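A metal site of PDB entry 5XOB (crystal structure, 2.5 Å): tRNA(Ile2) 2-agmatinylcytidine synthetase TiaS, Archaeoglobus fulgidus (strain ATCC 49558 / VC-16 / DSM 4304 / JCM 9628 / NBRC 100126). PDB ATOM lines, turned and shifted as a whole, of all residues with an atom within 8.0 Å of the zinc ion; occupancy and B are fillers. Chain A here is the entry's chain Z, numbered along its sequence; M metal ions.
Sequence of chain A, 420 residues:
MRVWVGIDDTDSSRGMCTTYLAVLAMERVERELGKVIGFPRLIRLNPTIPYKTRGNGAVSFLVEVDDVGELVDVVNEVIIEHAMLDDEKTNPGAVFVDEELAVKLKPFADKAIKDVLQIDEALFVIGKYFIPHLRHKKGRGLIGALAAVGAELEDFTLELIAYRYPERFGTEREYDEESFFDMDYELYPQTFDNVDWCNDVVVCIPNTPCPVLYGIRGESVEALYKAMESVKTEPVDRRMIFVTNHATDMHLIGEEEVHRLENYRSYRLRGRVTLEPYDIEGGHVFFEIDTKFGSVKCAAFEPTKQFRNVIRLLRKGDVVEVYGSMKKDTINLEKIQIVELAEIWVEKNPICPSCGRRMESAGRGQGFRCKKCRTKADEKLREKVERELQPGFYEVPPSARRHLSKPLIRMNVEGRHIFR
The side-chain sulfur (SG) of Cys 355 lies close to the backbone NH (N) of Arg 357 (3.4 Å). N of Cys 370 lies within hydrogen-bond range of O of Thr 375 (3.0 Å). The side-chain hydroxyl (OG) of Ser 354 lies close to the side-chain sulfur (SG) of Cys 373, at 3.4 Å. The side-chain sulfur (SG) of Cys 352 sits close to the backbone NH (N) of Ser 354, 3.6 Å away. The backbone carbonyl oxygen (O) of Arg 357 sits at hydrogen-bond distance from the backbone NH (N) of Cys 352, at 2.8 Å. The side-chain sulfur (SG) of Cys 352 lies close to the side-chain hydroxyl (OG1) of Thr 375 (3.1 Å).
Within 4 Å of the zinc ion: Cys 352, Cys 355, Cys 370 and Cys 373.
The zinc ion is bound by SG of Cys 355, SG of Cys 370, SG of Cys 352 and SG of Cys 373.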
ATOM      1  N   ILE A 351      -7.794  21.621  10.971  1.00  0.00           N
ATOM      2  CA  ILE A 351      -6.519  22.037  10.387  1.00  0.00           C
ATOM      3  C   ILE A 351      -5.563  20.856  10.467  1.00  0.00           C
ATOM      4  O   ILE A 351      -5.418  20.239  11.529  1.00  0.00           O
ATOM      5  CB  ILE A 351      -5.940  23.251  11.143  1.00  0.00           C
ATOM      6  CG1 ILE A 351      -6.898  24.455  11.086  1.00  0.00           C
ATOM      7  CG2 ILE A 351      -4.560  23.628  10.610  1.00  0.00           C
ATOM      8  CD1 ILE A 351      -7.291  24.909   9.682  1.00  0.00           C
ATOM      9  N   CYS A 352      -4.910  20.521   9.356  1.00  0.00           N
ATOM     10  CA  CYS A 352      -3.915  19.453   9.338  1.00  0.00           C
ATOM     11  C   CYS A 352      -2.745  19.769  10.279  1.00  0.00           C
ATOM     12  O   CYS A 352      -2.190  20.866  10.217  1.00  0.00           O
ATOM     13  CB  CYS A 352      -3.381  19.215   7.929  1.00  0.00           C
ATOM     14  SG  CYS A 352      -2.099  17.947   7.853  1.00  0.00           S
ATOM     15  N   PRO A 353      -2.351  18.810  11.136  1.00  0.00           N
ATOM     16  CA  PRO A 353      -1.337  19.070  12.159  1.00  0.00           C
ATOM     17  C   PRO A 353       0.080  19.187  11.602  1.00  0.00           C
ATOM     18  O   PRO A 353       0.932  19.841  12.211  1.00  0.00           O
ATOM     19  CB  PRO A 353      -1.428  17.835  13.072  1.00  0.00           C
ATOM     20  CG  PRO A 353      -2.564  17.017  12.569  1.00  0.00           C
ATOM     21  CD  PRO A 353      -2.759  17.402  11.138  1.00  0.00           C
ATOM     22  N   SER A 354       0.334  18.535  10.471  1.00  0.00           N
ATOM     23  CA  SER A 354       1.641  18.590   9.828  1.00  0.00           C
ATOM     24  C   SER A 354       1.811  19.881   9.039  1.00  0.00           C
ATOM     25  O   SER A 354       2.550  20.782   9.457  1.00  0.00           O
ATOM     26  CB  SER A 354       1.848  17.393   8.886  1.00  0.00           C
ATOM     27  OG  SER A 354       2.931  17.639   7.998  1.00  0.00           O
ATOM     28  N   CYS A 355       1.125  19.972   7.906  1.00  0.00           N
ATOM     29  CA  CYS A 355       1.329  21.089   6.979  1.00  0.00           C
ATOM     30  C   CYS A 355       0.560  22.354   7.385  1.00  0.00           C
ATOM     31  O   CYS A 355       0.872  23.448   6.916  1.00  0.00           O
ATOM     32  CB  CYS A 355       0.914  20.683   5.561  1.00  0.00           C
ATOM     33  SG  CYS A 355      -0.878  20.620   5.345  1.00  0.00           S
ATOM     34  N   GLY A 356      -0.457  22.211   8.237  1.00  0.00           N
ATOM     35  CA  GLY A 356      -1.205  23.356   8.734  1.00  0.00           C
ATOM     36  C   GLY A 356      -2.305  23.867   7.820  1.00  0.00           C
ATOM     37  O   GLY A 356      -2.987  24.833   8.182  1.00  0.00           O
ATOM     38  N   ARG A 357      -2.502  23.249   6.653  1.00  0.00           N
ATOM     39  CA  ARG A 357      -3.599  23.670   5.784  1.00  0.00           C
ATOM     40  C   ARG A 357      -4.909  23.035   6.248  1.00  0.00           C
ATOM     41  O   ARG A 357      -4.908  22.166   7.114  1.00  0.00           O
ATOM     42  CB  ARG A 357      -3.321  23.396   4.288  1.00  0.00           C
ATOM     43  CG  ARG A 357      -3.533  21.969   3.786  1.00  0.00           C
ATOM     44  CD  ARG A 357      -4.530  21.884   2.637  1.00  0.00           C
ATOM     45  NE  ARG A 357      -4.268  22.816   1.527  1.00  0.00           N
ATOM     46  CZ  ARG A 357      -5.021  22.920   0.432  1.00  0.00           C
ATOM     47  NH1 ARG A 357      -6.095  22.139   0.257  1.00  0.00           N
ATOM     48  NH2 ARG A 357      -4.704  23.801  -0.511  1.00  0.00           N
ATOM     49  N   ARG A 358      -6.013  23.473   5.664  1.00  0.00           N
ATOM     50  CA  ARG A 358      -7.334  22.954   6.007  1.00  0.00           C
ATOM     51  C   ARG A 358      -7.530  21.559   5.413  1.00  0.00           C
ATOM     52  O   ARG A 358      -7.235  21.329   4.246  1.00  0.00           O
ATOM     53  CB  ARG A 358      -8.414  23.898   5.482  1.00  0.00           C
ATOM     54  CG  ARG A 358      -9.755  23.791   6.184  1.00  0.00           C
ATOM     55  CD  ARG A 358     -10.862  24.338   5.296  1.00  0.00           C
ATOM     56  NE  ARG A 358     -11.162  23.404   4.207  1.00  0.00           N
ATOM     57  CZ  ARG A 358     -12.379  23.021   3.827  1.00  0.00           C
ATOM     58  NH1 ARG A 358     -12.487  22.153   2.832  1.00  0.00           N
ATOM     59  NH2 ARG A 358     -13.478  23.501   4.411  1.00  0.00           N
ATOM     60  N   MET A 359      -8.047  20.636   6.224  1.00  0.00           N
ATOM     61  CA  MET A 359      -8.343  19.285   5.757  1.00  0.00           C
ATOM     62  C   MET A 359      -9.586  19.295   4.863  1.00  0.00           C
ATOM     63  O   MET A 359     -10.587  19.928   5.199  1.00  0.00           O
ATOM     64  CB  MET A 359      -8.586  18.314   6.917  1.00  0.00           C
ATOM     65  CG  MET A 359      -7.331  17.777   7.599  1.00  0.00           C
ATOM     66  SD  MET A 359      -7.643  16.226   8.470  1.00  0.00           S
ATOM     67  CE  MET A 359      -6.022  15.879   9.114  1.00  0.00           C
ATOM     68  N   ARG A 369      -9.455  14.463   5.816  1.00  0.00           N
ATOM     69  CA  ARG A 369      -8.155  13.966   5.382  1.00  0.00           C
ATOM     70  C   ARG A 369      -7.277  15.125   4.935  1.00  0.00           C
ATOM     71  O   ARG A 369      -7.764  16.217   4.639  1.00  0.00           O
ATOM     72  CB  ARG A 369      -8.337  12.986   4.221  1.00  0.00           C
ATOM     73  N   CYS A 370      -5.980  14.874   4.889  1.00  0.00           N
ATOM     74  CA  CYS A 370      -5.055  15.736   4.180  1.00  0.00           C
ATOM     75  C   CYS A 370      -4.201  14.802   3.350  1.00  0.00           C
ATOM     76  O   CYS A 370      -3.372  14.093   3.883  1.00  0.00           O
ATOM     77  CB  CYS A 370      -4.197  16.535   5.136  1.00  0.00           C
ATOM     78  SG  CYS A 370      -2.703  17.210   4.384  1.00  0.00           S
ATOM     79  N   LYS A 371      -4.456  14.788   2.042  1.00  0.00           N
ATOM     80  CA  LYS A 371      -3.857  13.809   1.130  1.00  0.00           C
ATOM     81  C   LYS A 371      -2.353  13.998   0.893  1.00  0.00           C
ATOM     82  O   LYS A 371      -1.653  13.030   0.587  1.00  0.00           O
ATOM     83  CB  LYS A 371      -4.607  13.827  -0.206  1.00  0.00           C
ATOM     84  N   LYS A 372      -1.845  15.219   1.072  1.00  0.00           N
ATOM     85  CA  LYS A 372      -0.440  15.546   0.775  1.00  0.00           C
ATOM     86  C   LYS A 372       0.483  15.129   1.927  1.00  0.00           C
ATOM     87  O   LYS A 372       1.630  14.741   1.708  1.00  0.00           O
ATOM     88  CB  LYS A 372      -0.233  17.025   0.407  1.00  0.00           C
ATOM     89  CG  LYS A 372      -0.844  18.062   1.344  1.00  0.00           C
ATOM     90  CD  LYS A 372      -1.907  18.929   0.674  1.00  0.00           C
ATOM     91  CE  LYS A 372      -3.209  18.209   0.328  1.00  0.00           C
ATOM     92  NZ  LYS A 372      -4.361  18.533   1.229  1.00  0.00           N
ATOM     93  N   CYS A 373      -0.027  15.234   3.149  1.00  0.00           N
ATOM     94  CA  CYS A 373       0.501  14.460   4.268  1.00  0.00           C
ATOM     95  C   CYS A 373      -0.281  13.162   4.229  1.00  0.00           C
ATOM     96  O   CYS A 373      -0.971  12.899   3.245  1.00  0.00           O
ATOM     97  CB  CYS A 373       0.289  15.228   5.560  1.00  0.00           C
ATOM     98  SG  CYS A 373       0.876  16.937   5.413  1.00  0.00           S
ATOM     99  N   ARG A 374      -0.177  12.318   5.243  1.00  0.00           N
ATOM    100  CA  ARG A 374      -1.005  11.099   5.253  1.00  0.00           C
ATOM    101  C   ARG A 374      -1.954  11.136   6.460  1.00  0.00           C
ATOM    102  O   ARG A 374      -2.141  10.119   7.143  1.00  0.00           O
ATOM    103  CB  ARG A 374      -0.128   9.847   5.265  1.00  0.00           C
ATOM    104  N   THR A 375      -2.558  12.293   6.689  1.00  0.00           N
ATOM    105  CA  THR A 375      -3.219  12.569   7.969  1.00  0.00           C
ATOM    106  C   THR A 375      -4.758  12.560   7.913  1.00  0.00           C
ATOM    107  O   THR A 375      -5.366  12.653   6.847  1.00  0.00           O
ATOM    108  CB  THR A 375      -2.737  13.915   8.550  1.00  0.00           C
ATOM    109  OG1 THR A 375      -3.132  14.990   7.695  1.00  0.00           O
ATOM    110  CG2 THR A 375      -1.226  13.916   8.681  1.00  0.00           C
HETATM  111 ZN    ZN M   1      -1.117  18.495   5.672  1.00  0.00          ZN
